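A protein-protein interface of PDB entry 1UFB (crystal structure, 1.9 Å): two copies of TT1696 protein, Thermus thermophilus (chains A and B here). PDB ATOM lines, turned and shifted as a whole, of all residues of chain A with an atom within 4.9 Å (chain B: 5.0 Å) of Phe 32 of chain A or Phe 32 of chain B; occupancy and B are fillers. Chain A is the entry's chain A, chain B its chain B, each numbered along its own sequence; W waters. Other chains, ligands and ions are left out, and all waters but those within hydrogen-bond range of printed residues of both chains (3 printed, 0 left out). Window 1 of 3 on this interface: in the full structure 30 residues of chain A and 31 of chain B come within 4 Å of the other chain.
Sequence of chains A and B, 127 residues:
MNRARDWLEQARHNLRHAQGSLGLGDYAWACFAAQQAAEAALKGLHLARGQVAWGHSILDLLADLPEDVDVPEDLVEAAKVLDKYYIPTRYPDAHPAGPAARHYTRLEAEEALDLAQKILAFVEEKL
Water W3 lies within hydrogen-bond range of NH2 of Arg 90 of chain A (2.7 Å), OH of Tyr 86 of chain B (2.9 Å) and OH of Tyr 86 of chain A (3.3 Å). Water W1 lies within hydrogen-bond range of NH2 of Arg 90 of chain B (2.8 Å), OH of Tyr 86 of chain A (2.9 Å) and OH of Tyr 86 of chain B (3.3 Å). Water W2 bridges the backbone carbonyl oxygen (O) of Arg 90 of chain B (2.8 Å) and the side-chain amide nitrogen (NE2) of Gln 36 of chain A (3.3 Å).
The side-chain amide nitrogen of Gln 36 of chain B is in hydrogen-bond range of the side-chain amide oxygen of Gln 35 of chain B. O of Tyr 86 of chain B sits at hydrogen-bond distance from NH2 of Arg 90 of chain B, at 2.9 Å. NH2 of Arg 90 of chain A is in hydrogen-bond range of O of Tyr 86 of chain A (2.9 Å). The side-chain amide oxygen (OE1) of Gln 36 of chain A sits close to the side-chain amide oxygen (OE1) of Gln 35 of chain A (2.9 Å).
Hydrophobic or aromatic side chains of chain B within 4 Å of the printed part of chain A: Trp 29, Phe 32 and Tyr 86. Along chain B the printed residues that touch a printed residue of chain A span positions 29 to 90. Hydrophobic or aromatic side chains of chain A that line the printed part of chain B: Trp 29, Phe 32, Ala 33 and Tyr 86. Among the printed residues, no Asp or Glu carboxylate lies within 4 Å of a Lys or Arg side-chain nitrogen of the other chain.
Trp 29 of chain A touches Phe 32 of chain B, and with the chains exchanged Phe 32 of chain A touches Trp 29 of chain B. Trp 29 of chain A touches Gln 36 of chain B, and with the chains exchanged Gln 36 of chain A touches Trp 29 of chain B. Gln 36 of chain A touches Arg 90 of chain B, and with the chains exchanged Arg 90 of chain A touches Gln 36 of chain B. Tyr 86 of chain A touches its own counterpart, Tyr 86 of chain B. 13 positions are printed for both chains. Of the 11 pairs that touch across the chains among the printed residues, 11 have their exchanged pair printed and touching as well.
Among the printed residues, pairs that only touch across the chains: Trp 29 of chain A with Trp 29 of chain B (3.8 Å), Trp 29 of chain A with Phe 32 of chain B (3.4 Å), Trp 29 of chain A with Ala 33 of chain B (3.98 Å), Trp 29 of chain A with Gln 36 of chain B (3.97 Å), Phe 32 of chain A with Trp 29 of chain B (3.5 Å), Phe 32 of chain A with Phe 32 of chain B (3.7 Å), Ala 33 of chain A with Trp 29 of chain B (3.9 Å) and Gln 36 of chain A with Trp 29 of chain B (3.95 Å).
Printed residues of chain B within 4 Å of Phe 32 of chain A: Trp 29 and Phe 32. Of the printed residues of chain B, Tyr 86 of chain A touches Tyr 86 (3.4 Å). Phe 32 of chain B touches just these residues of chain A: Trp 29 (3.4 Å) and Phe 32 (3.7 Å). Printed residues of chain A within 4 Å of Ala 33 of chain B: Trp 29. The nearest residue of chain B that does not touch Phe 32 of chain A is Arg 90 of chain B (4.03 Å).
OE1 of Gln 36 of chain B lies within hydrogen-bond range of NH1 of Arg 90 of chain A, 2.9 Å away. OH of Tyr 86 of chain A is in hydrogen-bond range of OH of Tyr 86 of chain B. The side-chain amide nitrogen (NE2) of Gln 36 of chain A sits close to the guanidinium group (NH1) of Arg 90 of chain B, 2.9 Å away.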
ATOM      1  N   ALA A  28       6.226 -12.916   6.875  1.00  0.00           N
ATOM      2  CA  ALA A  28       6.098 -11.941   7.915  1.00  0.00           C
ATOM      3  C   ALA A  28       7.461 -11.209   8.034  1.00  0.00           C
ATOM      4  O   ALA A  28       7.511  -9.961   8.160  1.00  0.00           O
ATOM      5  CB  ALA A  28       5.741 -12.630   9.220  1.00  0.00           C
ATOM      6  N   TRP A  29       8.546 -11.956   8.063  1.00  0.00           N
ATOM      7  CA  TRP A  29       9.859 -11.285   8.173  1.00  0.00           C
ATOM      8  C   TRP A  29      10.102 -10.384   6.979  1.00  0.00           C
ATOM      9  O   TRP A  29      10.729  -9.337   7.120  1.00  0.00           O
ATOM     10  CB  TRP A  29      11.008 -12.332   8.302  1.00  0.00           C
ATOM     11  CG  TRP A  29      11.214 -12.678   9.759  1.00  0.00           C
ATOM     12  CD1 TRP A  29      10.705 -13.753  10.429  1.00  0.00           C
ATOM     13  CD2 TRP A  29      11.965 -11.916  10.721  1.00  0.00           C
ATOM     14  NE1 TRP A  29      11.100 -13.722  11.769  1.00  0.00           N
ATOM     15  CE2 TRP A  29      11.873 -12.601  11.973  1.00  0.00           C
ATOM     16  CE3 TRP A  29      12.713 -10.742  10.649  1.00  0.00           C
ATOM     17  CZ2 TRP A  29      12.516 -12.130  13.157  1.00  0.00           C
ATOM     18  CZ3 TRP A  29      13.361 -10.276  11.828  1.00  0.00           C
ATOM     19  CH2 TRP A  29      13.245 -10.979  13.064  1.00  0.00           C
ATOM     20  N   ALA A  30       9.647 -10.803   5.772  1.00  0.00           N
ATOM     21  CA  ALA A  30       9.807  -9.972   4.586  1.00  0.00           C
ATOM     22  C   ALA A  30       9.022  -8.659   4.767  1.00  0.00           C
ATOM     23  O   ALA A  30       9.462  -7.577   4.340  1.00  0.00           O
ATOM     24  CB  ALA A  30       9.255 -10.729   3.284  1.00  0.00           C
ATOM     25  N   CYS A  31       7.839  -8.738   5.347  1.00  0.00           N
ATOM     26  CA  CYS A  31       7.032  -7.564   5.562  1.00  0.00           C
ATOM     27  C   CYS A  31       7.715  -6.618   6.570  1.00  0.00           C
ATOM     28  O   CYS A  31       7.673  -5.392   6.423  1.00  0.00           O
ATOM     29  CB  CYS A  31       5.670  -7.920   6.167  1.00  0.00           C
ATOM     30  SG  CYS A  31       4.561  -8.703   4.861  1.00  0.00           S
ATOM     31  N   PHE A  32       8.273  -7.217   7.618  1.00  0.00           N
ATOM     32  CA  PHE A  32       8.976  -6.393   8.607  1.00  0.00           C
ATOM     33  C   PHE A  32      10.184  -5.693   7.938  1.00  0.00           C
ATOM     34  O   PHE A  32      10.386  -4.476   8.071  1.00  0.00           O
ATOM     35  CB  PHE A  32       9.438  -7.301   9.759  1.00  0.00           C
ATOM     36  CG  PHE A  32      10.309  -6.582  10.765  1.00  0.00           C
ATOM     37  CD1 PHE A  32       9.716  -5.675  11.638  1.00  0.00           C
ATOM     38  CD2 PHE A  32      11.697  -6.794  10.808  1.00  0.00           C
ATOM     39  CE1 PHE A  32      10.481  -4.977  12.569  1.00  0.00           C
ATOM     40  CE2 PHE A  32      12.516  -6.089  11.759  1.00  0.00           C
ATOM     41  CZ  PHE A  32      11.887  -5.186  12.627  1.00  0.00           C
ATOM     42  N   ALA A  33      10.950  -6.451   7.162  1.00  0.00           N
ATOM     43  CA  ALA A  33      12.111  -5.897   6.496  1.00  0.00           C
ATOM     44  C   ALA A  33      11.677  -4.810   5.521  1.00  0.00           C
ATOM     45  O   ALA A  33      12.372  -3.852   5.374  1.00  0.00           O
ATOM     46  CB  ALA A  33      12.973  -7.041   5.798  1.00  0.00           C
ATOM     47  N   ALA A  34      10.512  -4.928   4.881  1.00  0.00           N
ATOM     48  CA  ALA A  34      10.055  -3.880   3.980  1.00  0.00           C
ATOM     49  C   ALA A  34       9.720  -2.615   4.785  1.00  0.00           C
ATOM     50  O   ALA A  34      10.031  -1.472   4.388  1.00  0.00           O
ATOM     51  CB  ALA A  34       8.796  -4.359   3.192  1.00  0.00           C
ATOM     52  N   GLN A  35       9.018  -2.781   5.901  1.00  0.00           N
ATOM     53  CA  GLN A  35       8.749  -1.563   6.716  1.00  0.00           C
ATOM     54  C   GLN A  35      10.132  -0.937   7.146  1.00  0.00           C
ATOM     55  O   GLN A  35      10.273   0.303   7.181  1.00  0.00           O
ATOM     56  CB  GLN A  35       7.939  -1.938   7.996  1.00  0.00           C
ATOM     57  CG  GLN A  35       7.661  -0.762   8.988  1.00  0.00           C
ATOM     58  CD  GLN A  35       8.893  -0.400   9.878  1.00  0.00           C
ATOM     59  OE1 GLN A  35       9.764  -1.231  10.106  1.00  0.00           O
ATOM     60  NE2 GLN A  35       8.917   0.866  10.433  1.00  0.00           N
ATOM     61  N   GLN A  36      11.114  -1.787   7.464  1.00  0.00           N
ATOM     62  CA  GLN A  36      12.414  -1.286   7.906  1.00  0.00           C
ATOM     63  C   GLN A  36      13.137  -0.550   6.775  1.00  0.00           C
ATOM     64  O   GLN A  36      13.872   0.435   7.021  1.00  0.00           O
ATOM     65  CB  GLN A  36      13.283  -2.446   8.435  1.00  0.00           C
ATOM     66  CG  GLN A  36      12.877  -2.950   9.823  1.00  0.00           C
ATOM     67  CD  GLN A  36      13.220  -1.912  10.902  1.00  0.00           C
ATOM     68  OE1 GLN A  36      12.354  -1.084  11.393  1.00  0.00           O
ATOM     69  NE2 GLN A  36      14.482  -1.929  11.288  1.00  0.00           N
ATOM     70  N   TYR A  85       3.309  -3.373   9.900  1.00  0.00           N
ATOM     71  CA  TYR A  85       4.286  -4.488   9.831  1.00  0.00           C
ATOM     72  C   TYR A  85       5.459  -4.360  10.808  1.00  0.00           C
ATOM     73  O   TYR A  85       6.332  -5.237  10.803  1.00  0.00           O
ATOM     74  CB  TYR A  85       4.839  -4.643   8.404  1.00  0.00           C
ATOM     75  CG  TYR A  85       3.742  -4.972   7.371  1.00  0.00           C
ATOM     76  CD1 TYR A  85       3.857  -4.557   6.031  1.00  0.00           C
ATOM     77  CD2 TYR A  85       2.631  -5.723   7.738  1.00  0.00           C
ATOM     78  CE1 TYR A  85       2.871  -4.887   5.054  1.00  0.00           C
ATOM     79  CE2 TYR A  85       1.637  -6.075   6.763  1.00  0.00           C
ATOM     80  CZ  TYR A  85       1.783  -5.646   5.430  1.00  0.00           C
ATOM     81  OH  TYR A  85       0.886  -5.999   4.429  1.00  0.00           O
ATOM     82  N   TYR A  86       5.524  -3.265  11.581  1.00  0.00           N
ATOM     83  CA  TYR A  86       6.637  -3.133  12.502  1.00  0.00           C
ATOM     84  C   TYR A  86       6.524  -4.130  13.695  1.00  0.00           C
ATOM     85  O   TYR A  86       7.445  -4.892  13.986  1.00  0.00           O
ATOM     86  CB  TYR A  86       6.764  -1.670  12.978  1.00  0.00           C
ATOM     87  CG  TYR A  86       7.833  -1.507  14.028  1.00  0.00           C
ATOM     88  CD1 TYR A  86       9.198  -1.699  13.719  1.00  0.00           C
ATOM     89  CD2 TYR A  86       7.456  -1.308  15.387  1.00  0.00           C
ATOM     90  CE1 TYR A  86      10.195  -1.703  14.793  1.00  0.00           C
ATOM     91  CE2 TYR A  86       8.382  -1.328  16.403  1.00  0.00           C
ATOM     92  CZ  TYR A  86       9.734  -1.515  16.115  1.00  0.00           C
ATOM     93  OH  TYR A  86      10.567  -1.441  17.189  1.00  0.00           O
ATOM     94  N   THR A  89       4.181  -8.391  12.723  1.00  0.00           N
ATOM     95  CA  THR A  89       4.892  -9.429  11.998  1.00  0.00           C
ATOM     96  C   THR A  89       5.768 -10.298  12.888  1.00  0.00           C
ATOM     97  O   THR A  89       6.205 -11.347  12.482  1.00  0.00           O
ATOM     98  CB  THR A  89       5.791  -8.789  10.951  1.00  0.00           C
ATOM     99  OG1 THR A  89       6.530  -7.687  11.559  1.00  0.00           O
ATOM    100  CG2 THR A  89       4.928  -8.219   9.814  1.00  0.00           C
ATOM    101  N   ARG A  90       6.020  -9.883  14.125  1.00  0.00           N
ATOM    102  CA  ARG A  90       6.971 -10.598  15.003  1.00  0.00           C
ATOM    103  C   ARG A  90       6.400 -10.996  16.371  1.00  0.00           C
ATOM    104  O   ARG A  90       6.988 -11.819  17.057  1.00  0.00           O
ATOM    105  CB  ARG A  90       8.172  -9.684  15.324  1.00  0.00           C
ATOM    106  CG  ARG A  90       8.967  -9.229  14.088  1.00  0.00           C
ATOM    107  CD  ARG A  90      10.075  -8.264  14.507  1.00  0.00           C
ATOM    108  NE  ARG A  90       9.538  -6.952  14.863  1.00  0.00           N
ATOM    109  CZ  ARG A  90       9.883  -6.248  15.967  1.00  0.00           C
ATOM    110  NH1 ARG A  90      10.771  -6.726  16.886  1.00  0.00           N
ATOM    111  NH2 ARG A  90       9.443  -5.000  16.091  1.00  0.00           N
ATOM    112  N   ALA B  28      24.093  -9.337   9.699  1.00  0.00           N
ATOM    113  CA  ALA B  28      23.476  -8.402  10.702  1.00  0.00           C
ATOM    114  C   ALA B  28      21.986  -8.837  10.964  1.00  0.00           C
ATOM    115  O   ALA B  28      21.563  -8.907  12.100  1.00  0.00           O
ATOM    116  CB  ALA B  28      23.539  -6.981  10.148  1.00  0.00           C
ATOM    117  N   TRP B  29      21.210  -9.138   9.908  1.00  0.00           N
ATOM    118  CA  TRP B  29      19.820  -9.598  10.052  1.00  0.00           C
ATOM    119  C   TRP B  29      19.759 -10.951  10.747  1.00  0.00           C
ATOM    120  O   TRP B  29      18.852 -11.210  11.559  1.00  0.00           O
ATOM    121  CB  TRP B  29      19.132  -9.646   8.660  1.00  0.00           C
ATOM    122  CG  TRP B  29      18.530  -8.289   8.300  1.00  0.00           C
ATOM    123  CD1 TRP B  29      19.064  -7.310   7.461  1.00  0.00           C
ATOM    124  CD2 TRP B  29      17.261  -7.803   8.733  1.00  0.00           C
ATOM    125  NE1 TRP B  29      18.174  -6.263   7.363  1.00  0.00           N
ATOM    126  CE2 TRP B  29      17.065  -6.531   8.129  1.00  0.00           C
ATOM    127  CE3 TRP B  29      16.268  -8.322   9.573  1.00  0.00           C
ATOM    128  CZ2 TRP B  29      15.889  -5.746   8.346  1.00  0.00           C
ATOM    129  CZ3 TRP B  29      15.076  -7.548   9.785  1.00  0.00           C
ATOM    130  CH2 TRP B  29      14.916  -6.271   9.170  1.00  0.00           C
ATOM    131  N   ALA B  30      20.742 -11.822  10.505  1.00  0.00           N
ATOM    132  CA  ALA B  30      20.781 -13.114  11.203  1.00  0.00           C
ATOM    133  C   ALA B  30      20.983 -12.851  12.723  1.00  0.00           C
ATOM    134  O   ALA B  30      20.365 -13.500  13.536  1.00  0.00           O
ATOM    135  CB  ALA B  30      21.979 -14.016  10.675  1.00  0.00           C
ATOM    136  N   CYS B  31      21.874 -11.900  13.081  1.00  0.00           N
ATOM    137  CA  CYS B  31      22.116 -11.608  14.488  1.00  0.00           C
ATOM    138  C   CYS B  31      20.833 -11.057  15.145  1.00  0.00           C
ATOM    139  O   CYS B  31      20.459 -11.478  16.285  1.00  0.00           O
ATOM    140  CB  CYS B  31      23.268 -10.592  14.646  1.00  0.00           C
ATOM    141  SG  CYS B  31      24.866 -11.396  14.251  1.00  0.00           S
ATOM    142  N   PHE B  32      20.224 -10.095  14.462  1.00  0.00           N
ATOM    143  CA  PHE B  32      18.955  -9.548  14.967  1.00  0.00           C
ATOM    144  C   PHE B  32      17.896 -10.659  15.165  1.00  0.00           C
ATOM    145  O   PHE B  32      17.222 -10.703  16.183  1.00  0.00           O
ATOM    146  CB  PHE B  32      18.373  -8.552  13.993  1.00  0.00           C
ATOM    147  CG  PHE B  32      17.012  -8.054  14.397  1.00  0.00           C
ATOM    148  CD1 PHE B  32      16.868  -7.167  15.514  1.00  0.00           C
ATOM    149  CD2 PHE B  32      15.887  -8.448  13.688  1.00  0.00           C
ATOM    150  CE1 PHE B  32      15.604  -6.685  15.902  1.00  0.00           C
ATOM    151  CE2 PHE B  32      14.618  -7.978  14.071  1.00  0.00           C
ATOM    152  CZ  PHE B  32      14.494  -7.075  15.208  1.00  0.00           C
ATOM    153  N   ALA B  33      17.713 -11.527  14.161  1.00  0.00           N
ATOM    154  CA  ALA B  33      16.671 -12.583  14.311  1.00  0.00           C
ATOM    155  C   ALA B  33      16.998 -13.526  15.463  1.00  0.00           C
ATOM    156  O   ALA B  33      16.107 -14.074  16.088  1.00  0.00           O
ATOM    157  CB  ALA B  33      16.531 -13.394  12.982  1.00  0.00           C
ATOM    158  N   ALA B  34      18.290 -13.745  15.732  1.00  0.00           N
ATOM    159  CA  ALA B  34      18.690 -14.610  16.822  1.00  0.00           C
ATOM    160  C   ALA B  34      18.294 -13.965  18.141  1.00  0.00           C
ATOM    161  O   ALA B  34      17.834 -14.640  19.057  1.00  0.00           O
ATOM    162  CB  ALA B  34      20.226 -14.844  16.803  1.00  0.00           C
ATOM    163  N   GLN B  35      18.514 -12.665  18.269  1.00  0.00           N
ATOM    164  CA  GLN B  35      18.090 -11.998  19.486  1.00  0.00           C
ATOM    165  C   GLN B  35      16.521 -12.133  19.608  1.00  0.00           C
ATOM    166  O   GLN B  35      15.970 -12.297  20.723  1.00  0.00           O
ATOM    167  CB  GLN B  35      18.482 -10.515  19.430  1.00  0.00           C
ATOM    168  CG  GLN B  35      18.062  -9.639  20.687  1.00  0.00           C
ATOM    169  CD  GLN B  35      16.570  -9.199  20.611  1.00  0.00           C
ATOM    170  OE1 GLN B  35      15.998  -9.155  19.525  1.00  0.00           O
ATOM    171  NE2 GLN B  35      15.960  -8.873  21.760  1.00  0.00           N
ATOM    172  N   GLN B  36      15.811 -12.012  18.474  1.00  0.00           N
ATOM    173  CA  GLN B  36      14.365 -12.118  18.496  1.00  0.00           C
ATOM    174  C   GLN B  36      13.914 -13.555  18.871  1.00  0.00           C
ATOM    175  O   GLN B  36      12.870 -13.722  19.506  1.00  0.00           O
ATOM    176  CB  GLN B  36      13.770 -11.684  17.127  1.00  0.00           C
ATOM    177  CG  GLN B  36      13.845 -10.182  16.904  1.00  0.00           C
ATOM    178  CD  GLN B  36      12.773  -9.438  17.695  1.00  0.00           C
ATOM    179  OE1 GLN B  36      11.580  -9.432  17.311  1.00  0.00           O
ATOM    180  NE2 GLN B  36      13.179  -8.817  18.817  1.00  0.00           N
ATOM    181  N   TYR B  85      22.382  -7.029  19.727  1.00  0.00           N
ATOM    182  CA  TYR B  85      21.960  -7.182  18.353  1.00  0.00           C
ATOM    183  C   TYR B  85      20.554  -6.684  18.138  1.00  0.00           C
ATOM    184  O   TYR B  85      20.048  -6.826  17.024  1.00  0.00           O
ATOM    185  CB  TYR B  85      22.000  -8.643  17.946  1.00  0.00           C
ATOM    186  CG  TYR B  85      23.388  -9.277  18.014  1.00  0.00           C
ATOM    187  CD1 TYR B  85      23.526 -10.593  18.350  1.00  0.00           C
ATOM    188  CD2 TYR B  85      24.546  -8.530  17.710  1.00  0.00           C
ATOM    189  CE1 TYR B  85      24.813 -11.193  18.373  1.00  0.00           C
ATOM    190  CE2 TYR B  85      25.825  -9.117  17.728  1.00  0.00           C
ATOM    191  CZ  TYR B  85      25.929 -10.437  18.063  1.00  0.00           C
ATOM    192  OH  TYR B  85      27.181 -11.016  18.098  1.00  0.00           O
ATOM    193  N   TYR B  86      19.900  -6.167  19.166  1.00  0.00           N
ATOM    194  CA  TYR B  86      18.535  -5.697  18.946  1.00  0.00           C
ATOM    195  C   TYR B  86      18.520  -4.403  18.060  1.00  0.00           C
ATOM    196  O   TYR B  86      17.824  -4.339  17.033  1.00  0.00           O
ATOM    197  CB  TYR B  86      17.787  -5.474  20.288  1.00  0.00           C
ATOM    198  CG  TYR B  86      16.414  -4.866  20.056  1.00  0.00           C
ATOM    199  CD1 TYR B  86      15.392  -5.615  19.443  1.00  0.00           C
ATOM    200  CD2 TYR B  86      16.148  -3.523  20.422  1.00  0.00           C
ATOM    201  CE1 TYR B  86      14.099  -4.996  19.185  1.00  0.00           C
ATOM    202  CE2 TYR B  86      14.929  -2.917  20.170  1.00  0.00           C
ATOM    203  CZ  TYR B  86      13.912  -3.659  19.546  1.00  0.00           C
ATOM    204  OH  TYR B  86      12.760  -2.984  19.242  1.00  0.00           O
ATOM    205  N   THR B  89      22.319  -3.907  14.788  1.00  0.00           N
ATOM    206  CA  THR B  89      22.272  -4.663  13.541  1.00  0.00           C
ATOM    207  C   THR B  89      21.426  -4.000  12.437  1.00  0.00           C
ATOM    208  O   THR B  89      21.515  -4.411  11.289  1.00  0.00           O
ATOM    209  CB  THR B  89      21.610  -6.007  13.796  1.00  0.00           C
ATOM    210  OG1 THR B  89      20.381  -5.771  14.507  1.00  0.00           O
ATOM    211  CG2 THR B  89      22.525  -6.899  14.681  1.00  0.00           C
ATOM    212  N   ARG B  90      20.602  -3.006  12.797  1.00  0.00           N
ATOM    213  CA  ARG B  90      19.683  -2.373  11.849  1.00  0.00           C
ATOM    214  C   ARG B  90      19.831  -0.890  11.713  1.00  0.00           C
ATOM    215  O   ARG B  90      19.378  -0.321  10.726  1.00  0.00           O
ATOM    216  CB  ARG B  90      18.228  -2.602  12.331  1.00  0.00           C
ATOM    217  CG  ARG B  90      17.838  -4.112  12.381  1.00  0.00           C
ATOM    218  CD  ARG B  90      16.415  -4.364  12.978  1.00  0.00           C
ATOM    219  NE  ARG B  90      16.283  -3.982  14.420  1.00  0.00           N
ATOM    220  CZ  ARG B  90      15.374  -3.153  14.935  1.00  0.00           C
ATOM    221  NH1 ARG B  90      14.473  -2.504  14.171  1.00  0.00           N
ATOM    222  NH2 ARG B  90      15.275  -3.070  16.287  1.00  0.00           N
HETATM  223  O   HOH W   1      13.430  -1.057  16.646  1.00  0.00           O
HETATM  224  O   HOH W   2      16.881  -0.554   9.533  1.00  0.00           O
HETATM  225  O   HOH W   3      10.317  -4.361  18.615  1.00  0.00           O
